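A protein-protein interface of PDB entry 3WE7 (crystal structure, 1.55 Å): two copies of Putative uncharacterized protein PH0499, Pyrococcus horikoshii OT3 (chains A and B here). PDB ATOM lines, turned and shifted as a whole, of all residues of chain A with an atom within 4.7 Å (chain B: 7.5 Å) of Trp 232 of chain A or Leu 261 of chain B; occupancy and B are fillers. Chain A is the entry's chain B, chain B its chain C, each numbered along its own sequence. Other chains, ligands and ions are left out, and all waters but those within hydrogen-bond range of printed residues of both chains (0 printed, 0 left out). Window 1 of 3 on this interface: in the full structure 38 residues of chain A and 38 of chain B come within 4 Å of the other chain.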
ATOM      1  N   ILE A  50      22.348  -1.607 -28.283  1.00  0.00           N
ATOM      2  CA  ILE A  50      21.334  -1.749 -27.243  1.00  0.00           C
ATOM      3  C   ILE A  50      21.929  -1.682 -25.856  1.00  0.00           C
ATOM      4  O   ILE A  50      21.395  -1.013 -24.967  1.00  0.00           O
ATOM      5  CB  ILE A  50      20.503  -3.014 -27.434  1.00  0.00           C
ATOM      6  CG1 ILE A  50      19.682  -2.908 -28.742  1.00  0.00           C
ATOM      7  CG2 ILE A  50      19.604  -3.321 -26.211  1.00  0.00           C
ATOM      8  CD1 ILE A  50      19.097  -4.269 -29.114  1.00  0.00           C
ATOM      9  N   PHE A 224      13.124  -4.269 -35.465  1.00  0.00           N
ATOM     10  CA  PHE A 224      12.228  -3.362 -34.760  1.00  0.00           C
ATOM     11  C   PHE A 224      11.159  -2.726 -35.638  1.00  0.00           C
ATOM     12  O   PHE A 224      11.072  -1.486 -35.725  1.00  0.00           O
ATOM     13  CB  PHE A 224      13.078  -2.258 -34.009  1.00  0.00           C
ATOM     14  CG  PHE A 224      14.026  -2.867 -32.977  1.00  0.00           C
ATOM     15  CD1 PHE A 224      13.479  -3.482 -31.890  1.00  0.00           C
ATOM     16  CD2 PHE A 224      15.440  -2.967 -33.186  1.00  0.00           C
ATOM     17  CE1 PHE A 224      14.294  -4.136 -30.916  1.00  0.00           C
ATOM     18  CE2 PHE A 224      16.227  -3.607 -32.231  1.00  0.00           C
ATOM     19  CZ  PHE A 224      15.688  -4.194 -31.110  1.00  0.00           C
ATOM     20  N   ILE A 228       6.806  -4.267 -32.766  1.00  0.00           N
ATOM     21  CA  ILE A 228       7.820  -4.737 -31.784  1.00  0.00           C
ATOM     22  C   ILE A 228       8.319  -3.497 -30.986  1.00  0.00           C
ATOM     23  O   ILE A 228       8.453  -3.559 -29.751  1.00  0.00           O
ATOM     24  CB  ILE A 228       8.996  -5.420 -32.522  1.00  0.00           C
ATOM     25  CG1 ILE A 228       8.511  -6.711 -33.237  1.00  0.00           C
ATOM     26  CG2 ILE A 228      10.224  -5.619 -31.610  1.00  0.00           C
ATOM     27  CD1 ILE A 228       8.022  -7.826 -32.348  1.00  0.00           C
ATOM     28  N   TRP A 229       8.532  -2.405 -31.693  1.00  0.00           N
ATOM     29  CA  TRP A 229       9.002  -1.178 -31.036  1.00  0.00           C
ATOM     30  C   TRP A 229       8.050  -0.623 -30.007  1.00  0.00           C
ATOM     31  O   TRP A 229       8.442   0.039 -29.018  1.00  0.00           O
ATOM     32  CB  TRP A 229       9.305  -0.133 -32.111  1.00  0.00           C
ATOM     33  CG  TRP A 229      10.149   1.020 -31.661  1.00  0.00           C
ATOM     34  CD1 TRP A 229       9.830   2.378 -31.588  1.00  0.00           C
ATOM     35  CD2 TRP A 229      11.514   0.935 -31.179  1.00  0.00           C
ATOM     36  NE1 TRP A 229      10.910   3.111 -31.157  1.00  0.00           N
ATOM     37  CE2 TRP A 229      11.952   2.311 -30.901  1.00  0.00           C
ATOM     38  CE3 TRP A 229      12.427  -0.120 -31.017  1.00  0.00           C
ATOM     39  CZ2 TRP A 229      13.254   2.597 -30.418  1.00  0.00           C
ATOM     40  CZ3 TRP A 229      13.715   0.191 -30.555  1.00  0.00           C
ATOM     41  CH2 TRP A 229      14.109   1.510 -30.255  1.00  0.00           C
ATOM     42  N   GLU A 230       6.737  -0.834 -30.192  1.00  0.00           N
ATOM     43  CA  GLU A 230       5.745  -0.451 -29.186  1.00  0.00           C
ATOM     44  C   GLU A 230       6.039  -1.045 -27.784  1.00  0.00           C
ATOM     45  O   GLU A 230       5.617  -0.452 -26.801  1.00  0.00           O
ATOM     46  CB  GLU A 230       4.405  -1.012 -29.689  1.00  0.00           C
ATOM     47  CG  GLU A 230       3.163  -0.724 -28.867  1.00  0.00           C
ATOM     48  CD  GLU A 230       1.878  -1.098 -29.658  1.00  0.00           C
ATOM     49  OE1 GLU A 230       0.781  -1.102 -29.054  1.00  0.00           O
ATOM     50  OE2 GLU A 230       1.969  -1.380 -30.894  1.00  0.00           O
ATOM     51  N   LYS A 231       6.665  -2.253 -27.743  1.00  0.00           N
ATOM     52  CA  LYS A 231       7.041  -2.880 -26.488  1.00  0.00           C
ATOM     53  C   LYS A 231       8.503  -2.501 -26.223  1.00  0.00           C
ATOM     54  O   LYS A 231       8.847  -2.244 -25.027  1.00  0.00           O
ATOM     55  CB  LYS A 231       6.870  -4.443 -26.510  1.00  0.00           C
ATOM     56  CG  LYS A 231       5.477  -4.938 -26.961  1.00  0.00           C
ATOM     57  CD  LYS A 231       4.342  -4.227 -26.257  1.00  0.00           C
ATOM     58  CE  LYS A 231       2.934  -4.667 -26.718  1.00  0.00           C
ATOM     59  NZ  LYS A 231       1.946  -3.927 -25.856  1.00  0.00           N
ATOM     60  N   TRP A 232       9.360  -2.500 -27.258  1.00  0.00           N
ATOM     61  CA  TRP A 232      10.832  -2.350 -26.962  1.00  0.00           C
ATOM     62  C   TRP A 232      11.240  -0.969 -26.570  1.00  0.00           C
ATOM     63  O   TRP A 232      12.169  -0.814 -25.739  1.00  0.00           O
ATOM     64  CB  TRP A 232      11.654  -2.878 -28.134  1.00  0.00           C
ATOM     65  CG  TRP A 232      11.898  -4.359 -27.980  1.00  0.00           C
ATOM     66  CD1 TRP A 232      11.022  -5.396 -28.215  1.00  0.00           C
ATOM     67  CD2 TRP A 232      13.125  -4.967 -27.506  1.00  0.00           C
ATOM     68  NE1 TRP A 232      11.640  -6.607 -27.939  1.00  0.00           N
ATOM     69  CE2 TRP A 232      12.908  -6.399 -27.470  1.00  0.00           C
ATOM     70  CE3 TRP A 232      14.370  -4.460 -27.091  1.00  0.00           C
ATOM     71  CZ2 TRP A 232      13.898  -7.275 -27.040  1.00  0.00           C
ATOM     72  CZ3 TRP A 232      15.352  -5.364 -26.683  1.00  0.00           C
ATOM     73  CH2 TRP A 232      15.123  -6.735 -26.668  1.00  0.00           C
ATOM     74  N   GLU A 233      10.585   0.080 -27.090  1.00  0.00           N
ATOM     75  CA  GLU A 233      10.992   1.446 -26.705  1.00  0.00           C
ATOM     76  C   GLU A 233      10.788   1.684 -25.203  1.00  0.00           C
ATOM     77  O   GLU A 233      11.760   2.093 -24.515  1.00  0.00           O
ATOM     78  CB  GLU A 233      10.314   2.526 -27.603  1.00  0.00           C
ATOM     79  CG  GLU A 233      11.119   3.828 -27.595  1.00  0.00           C
ATOM     80  CD  GLU A 233      10.365   5.067 -28.065  1.00  0.00           C
ATOM     81  OE1 GLU A 233       9.395   4.962 -28.832  1.00  0.00           O
ATOM     82  OE2 GLU A 233      10.741   6.186 -27.673  1.00  0.00           O
ATOM     83  N   PRO A 234       9.583   1.365 -24.651  1.00  0.00           N
ATOM     84  CA  PRO A 234       9.321   1.504 -23.158  1.00  0.00           C
ATOM     85  C   PRO A 234      10.274   0.575 -22.407  1.00  0.00           C
ATOM     86  O   PRO A 234      10.840   0.989 -21.357  1.00  0.00           O
ATOM     87  CB  PRO A 234       7.850   1.021 -22.976  1.00  0.00           C
ATOM     88  CG  PRO A 234       7.248   1.139 -24.320  1.00  0.00           C
ATOM     89  CD  PRO A 234       8.289   1.069 -25.365  1.00  0.00           C
ATOM     90  N   PHE A 235      10.617  -0.565 -22.971  1.00  0.00           N
ATOM     91  CA  PHE A 235      11.480  -1.531 -22.231  1.00  0.00           C
ATOM     92  C   PHE A 235      12.874  -0.973 -22.152  1.00  0.00           C
ATOM     93  O   PHE A 235      13.464  -0.922 -21.058  1.00  0.00           O
ATOM     94  CB  PHE A 235      11.468  -2.834 -23.019  1.00  0.00           C
ATOM     95  CG  PHE A 235      12.416  -3.907 -22.545  1.00  0.00           C
ATOM     96  CD1 PHE A 235      12.316  -4.506 -21.285  1.00  0.00           C
ATOM     97  CD2 PHE A 235      13.364  -4.409 -23.426  1.00  0.00           C
ATOM     98  CE1 PHE A 235      13.090  -5.607 -20.955  1.00  0.00           C
ATOM     99  CE2 PHE A 235      14.201  -5.474 -23.071  1.00  0.00           C
ATOM    100  CZ  PHE A 235      14.038  -6.108 -21.815  1.00  0.00           C
ATOM    101  N   LEU A 236      13.340  -0.446 -23.265  1.00  0.00           N
ATOM    102  CA  LEU A 236      14.758   0.067 -23.268  1.00  0.00           C
ATOM    103  C   LEU A 236      14.821   1.341 -22.419  1.00  0.00           C
ATOM    104  O   LEU A 236      15.870   1.545 -21.740  1.00  0.00           O
ATOM    105  CB  LEU A 236      15.181   0.458 -24.686  1.00  0.00           C
ATOM    106  CG  LEU A 236      15.330  -0.792 -25.620  1.00  0.00           C
ATOM    107  CD1 LEU A 236      15.329  -0.410 -27.106  1.00  0.00           C
ATOM    108  CD2 LEU A 236      16.604  -1.504 -25.339  1.00  0.00           C
ATOM    109  N   LEU B  19       5.552  -0.126 -17.498  1.00  0.00           N
ATOM    110  CA  LEU B  19       6.017  -1.189 -18.360  1.00  0.00           C
ATOM    111  C   LEU B  19       5.389  -2.525 -18.018  1.00  0.00           C
ATOM    112  O   LEU B  19       4.904  -3.198 -18.941  1.00  0.00           O
ATOM    113  CB  LEU B  19       7.572  -1.289 -18.249  1.00  0.00           C
ATOM    114  CG  LEU B  19       8.138  -2.408 -19.130  1.00  0.00           C
ATOM    115  CD1 LEU B  19       8.112  -2.088 -20.678  1.00  0.00           C
ATOM    116  CD2 LEU B  19       9.554  -2.651 -18.566  1.00  0.00           C
ATOM    117  N   VAL B  23       2.258  -1.741 -20.604  1.00  0.00           N
ATOM    118  CA  VAL B  23       2.911  -2.103 -21.848  1.00  0.00           C
ATOM    119  C   VAL B  23       2.919  -3.615 -22.011  1.00  0.00           C
ATOM    120  O   VAL B  23       2.590  -4.109 -23.071  1.00  0.00           O
ATOM    121  CB  VAL B  23       4.400  -1.520 -21.954  1.00  0.00           C
ATOM    122  CG1 VAL B  23       5.076  -2.011 -23.256  1.00  0.00           C
ATOM    123  CG2 VAL B  23       4.433   0.013 -21.811  1.00  0.00           C
ATOM    124  N   LEU B  24       3.272  -4.369 -20.974  1.00  0.00           N
ATOM    125  CA  LEU B  24       3.419  -5.814 -21.131  1.00  0.00           C
ATOM    126  C   LEU B  24       2.156  -6.552 -20.681  1.00  0.00           C
ATOM    127  O   LEU B  24       2.112  -7.792 -20.760  1.00  0.00           O
ATOM    128  CB  LEU B  24       4.664  -6.275 -20.365  1.00  0.00           C
ATOM    129  CG  LEU B  24       5.924  -5.600 -20.908  1.00  0.00           C
ATOM    130  CD1 LEU B  24       7.092  -6.111 -20.071  1.00  0.00           C
ATOM    131  CD2 LEU B  24       6.145  -6.035 -22.353  1.00  0.00           C
ATOM    132  N   MET B 258       7.082 -14.878 -15.914  1.00  0.00           N
ATOM    133  CA  MET B 258       7.532 -13.534 -16.240  1.00  0.00           C
ATOM    134  C   MET B 258       7.079 -13.153 -17.608  1.00  0.00           C
ATOM    135  O   MET B 258       6.848 -14.048 -18.414  1.00  0.00           O
ATOM    136  CB  MET B 258       9.071 -13.437 -16.276  1.00  0.00           C
ATOM    137  CG  MET B 258       9.665 -13.949 -14.959  1.00  0.00           C
ATOM    138  SD  MET B 258      11.443 -13.440 -14.782  1.00  0.00           S
ATOM    139  CE  MET B 258      12.256 -14.295 -16.119  1.00  0.00           C
ATOM    140  N   PRO B 259       7.058 -11.832 -17.902  1.00  0.00           N
ATOM    141  CA  PRO B 259       6.830 -11.407 -19.279  1.00  0.00           C
ATOM    142  C   PRO B 259       7.958 -11.994 -20.131  1.00  0.00           C
ATOM    143  O   PRO B 259       9.099 -12.173 -19.690  1.00  0.00           O
ATOM    144  CB  PRO B 259       7.016  -9.892 -19.235  1.00  0.00           C
ATOM    145  CG  PRO B 259       6.815  -9.475 -17.771  1.00  0.00           C
ATOM    146  CD  PRO B 259       7.220 -10.679 -16.981  1.00  0.00           C
ATOM    147  N   GLY B 260       7.624 -12.306 -21.376  1.00  0.00           N
ATOM    148  CA  GLY B 260       8.651 -12.802 -22.282  1.00  0.00           C
ATOM    149  C   GLY B 260       9.936 -11.953 -22.357  1.00  0.00           C
ATOM    150  O   GLY B 260      11.004 -12.539 -22.472  1.00  0.00           O
ATOM    151  N   LEU B 261       9.764 -10.624 -22.367  1.00  0.00           N
ATOM    152  CA  LEU B 261      10.981  -9.734 -22.511  1.00  0.00           C
ATOM    153  C   LEU B 261      11.917  -9.935 -21.358  1.00  0.00           C
ATOM    154  O   LEU B 261      13.129  -9.706 -21.541  1.00  0.00           O
ATOM    155  CB  LEU B 261      10.580  -8.244 -22.587  1.00  0.00           C
ATOM    156  CG  LEU B 261       9.738  -7.792 -23.816  1.00  0.00           C
ATOM    157  CD1 LEU B 261       9.798  -6.264 -23.762  1.00  0.00           C
ATOM    158  CD2 LEU B 261      10.250  -8.296 -25.156  1.00  0.00           C
ATOM    159  N   PHE B 262      11.405 -10.367 -20.211  1.00  0.00           N
ATOM    160  CA  PHE B 262      12.260 -10.460 -19.003  1.00  0.00           C
ATOM    161  C   PHE B 262      13.252 -11.633 -19.065  1.00  0.00           C
ATOM    162  O   PHE B 262      14.149 -11.707 -18.203  1.00  0.00           O
ATOM    163  CB  PHE B 262      11.425 -10.577 -17.716  1.00  0.00           C
ATOM    164  CG  PHE B 262      10.884  -9.277 -17.214  1.00  0.00           C
ATOM    165  CD1 PHE B 262      10.630  -8.219 -18.079  1.00  0.00           C
ATOM    166  CD2 PHE B 262      10.665  -9.128 -15.848  1.00  0.00           C
ATOM    167  CE1 PHE B 262      10.087  -6.989 -17.600  1.00  0.00           C
ATOM    168  CE2 PHE B 262      10.149  -7.902 -15.347  1.00  0.00           C
ATOM    169  CZ  PHE B 262       9.878  -6.864 -16.231  1.00  0.00           C
ATOM    170  N   TYR B 263      13.075 -12.567 -19.986  1.00  0.00           N
ATOM    171  CA  TYR B 263      14.030 -13.641 -20.201  1.00  0.00           C
ATOM    172  C   TYR B 263      15.255 -13.216 -20.996  1.00  0.00           C
ATOM    173  O   TYR B 263      16.043 -14.075 -21.444  1.00  0.00           O
ATOM    174  CB  TYR B 263      13.354 -14.836 -20.890  1.00  0.00           C
ATOM    175  CG  TYR B 263      12.350 -15.560 -19.964  1.00  0.00           C
ATOM    176  CD1 TYR B 263      12.733 -16.657 -19.220  1.00  0.00           C
ATOM    177  CD2 TYR B 263      11.017 -15.133 -19.872  1.00  0.00           C
ATOM    178  CE1 TYR B 263      11.813 -17.306 -18.404  1.00  0.00           C
ATOM    179  CE2 TYR B 263      10.105 -15.813 -19.113  1.00  0.00           C
ATOM    180  CZ  TYR B 263      10.531 -16.849 -18.342  1.00  0.00           C
ATOM    181  OH  TYR B 263       9.659 -17.608 -17.595  1.00  0.00           O
ATOM    182  N   HIS B 264      15.405 -11.938 -21.178  1.00  0.00           N
ATOM    183  CA  HIS B 264      16.541 -11.446 -21.969  1.00  0.00           C
ATOM    184  C   HIS B 264      16.938 -10.037 -21.661  1.00  0.00           C
ATOM    185  O   HIS B 264      16.076  -9.158 -21.528  1.00  0.00           O
ATOM    186  CB  HIS B 264      16.102 -11.528 -23.464  1.00  0.00           C
ATOM    187  CG  HIS B 264      17.225 -11.382 -24.472  1.00  0.00           C
ATOM    188  ND1 HIS B 264      18.373 -12.098 -24.410  1.00  0.00           N
ATOM    189  CD2 HIS B 264      17.338 -10.557 -25.595  1.00  0.00           C
ATOM    190  CE1 HIS B 264      19.171 -11.806 -25.421  1.00  0.00           C
ATOM    191  NE2 HIS B 264      18.564 -10.826 -26.164  1.00  0.00           N
ATOM    192  N   ILE B 265      18.273  -9.863 -21.377  1.00  0.00           N
ATOM    193  CA  ILE B 265      18.899  -8.540 -21.108  1.00  0.00           C
ATOM    194  C   ILE B 265      18.252  -7.726 -19.963  1.00  0.00           C
ATOM    195  O   ILE B 265      18.505  -6.555 -19.800  1.00  0.00           O
ATOM    196  CB  ILE B 265      19.123  -7.675 -22.391  1.00  0.00           C
ATOM    197  CG1 ILE B 265      17.799  -7.051 -22.918  1.00  0.00           C
ATOM    198  CG2 ILE B 265      19.840  -8.542 -23.469  1.00  0.00           C
ATOM    199  CD1 ILE B 265      18.116  -5.979 -23.980  1.00  0.00           C
ATOM    200  N   THR B 266      17.518  -8.367 -19.062  1.00  0.00           N
ATOM    201  CA  THR B 266      16.717  -7.572 -18.139  1.00  0.00           C
ATOM    202  C   THR B 266      17.432  -7.569 -16.738  1.00  0.00           C
ATOM    203  O   THR B 266      17.602  -8.604 -16.142  1.00  0.00           O
ATOM    204  CB  THR B 266      15.277  -8.250 -17.981  1.00  0.00           C
ATOM    205  OG1 THR B 266      14.640  -8.126 -19.267  1.00  0.00           O
ATOM    206  CG2 THR B 266      14.456  -7.437 -16.947  1.00  0.00           C
ATOM    207  N   THR B 269      14.871  -8.423 -12.956  1.00  0.00           N
ATOM    208  CA  THR B 269      13.973  -9.594 -12.914  1.00  0.00           C
ATOM    209  C   THR B 269      13.613  -9.920 -11.478  1.00  0.00           C
ATOM    210  O   THR B 269      12.586 -10.555 -11.254  1.00  0.00           O
ATOM    211  CB  THR B 269      14.568 -10.867 -13.500  1.00  0.00           C
ATOM    212  OG1 THR B 269      15.830 -11.132 -12.869  1.00  0.00           O
ATOM    213  CG2 THR B 269      14.754 -10.635 -15.051  1.00  0.00           C
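CG2 of Ile 50 of chain A touches CD1 of Ile 265 of chain B (3.8 Å).
Glu 230 of chain A touches Val 23 of chain B.
CD2 of Leu 261 of chain B touches NE1 of Trp 232 of chain A, 3.5 Å away.
Ile 265 of chain B touches Trp 232 of chain A.
Pro 234 of chain A touches Leu 19 of chain B (C to CD1, 3.8 Å).
Pro 234 of chain A touches Val 23 of chain B.
Phe 235 of chain A touches Leu 19 of chain B (N to CD1, 3.7 Å).
Phe 235 of chain A touches Leu 261 of chain B.
CZ of Phe 235 of chain A touches O of His 264 of chain B, at 3.7 Å.
Phe 235 of chain A touches Thr 266 of chain B (CZ to OG1, 3.3 Å).
The side-chain amino group of Lys 231 of chain A is in hydrogen-bond range of the backbone carbonyl oxygen of Val 23 of chain B (2.9 Å).
The backbone carbonyl oxygen (O) of Leu 261 of chain B sits at hydrogen-bond distance from the side-chain hydroxyl (OG1) of Thr 266 of chain B (3.2 Å).
The backbone carbonyl oxygen (O) of His 264 of chain B lies within hydrogen-bond range of the side-chain hydroxyl (OG1) of Thr 266 of chain B, at 2.9 Å.
The backbone carbonyl oxygen of Leu 19 of chain B is in hydrogen-bond range of the backbone NH of Leu 24 of chain B, at 2.9 Å.
No position is printed for both chains.
Printed residues of chain B within 4 Å of Ile 50 of chain A: Ile 265 (3.8 Å).
Of the printed residues of chain B, Glu 230 of chain A touches Val 23 (3.9 Å).
Printed residues of chain B within 4 Å of Lys 231 of chain A: Val 23.
Trp 232 of chain A touches just these residues of chain B: Leu 261 (3.5 Å) and Ile 265 (3.9 Å).
Of the printed residues of chain A, Leu 19 of chain B touches Pro 234 and Phe 235.
Leu 261 of chain B touches just these residues of chain A: Trp 232 and Phe 235.
Of the printed residues of chain A, Thr 266 of chain B touches Phe 235 (3.3 Å).
The nearest residue of chain A that does not touch Leu 261 of chain B is Lys 231 of chain A (4.3 Å).
The nearest printed residue of chain B that does not touch Ile 50 of chain A is His 264 of chain B (7.2 Å).
Hydrophobic or aromatic side chains of chain A within 4 Å of the printed part of chain B: Ile 50, Trp 232, Pro 234 and Phe 235.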
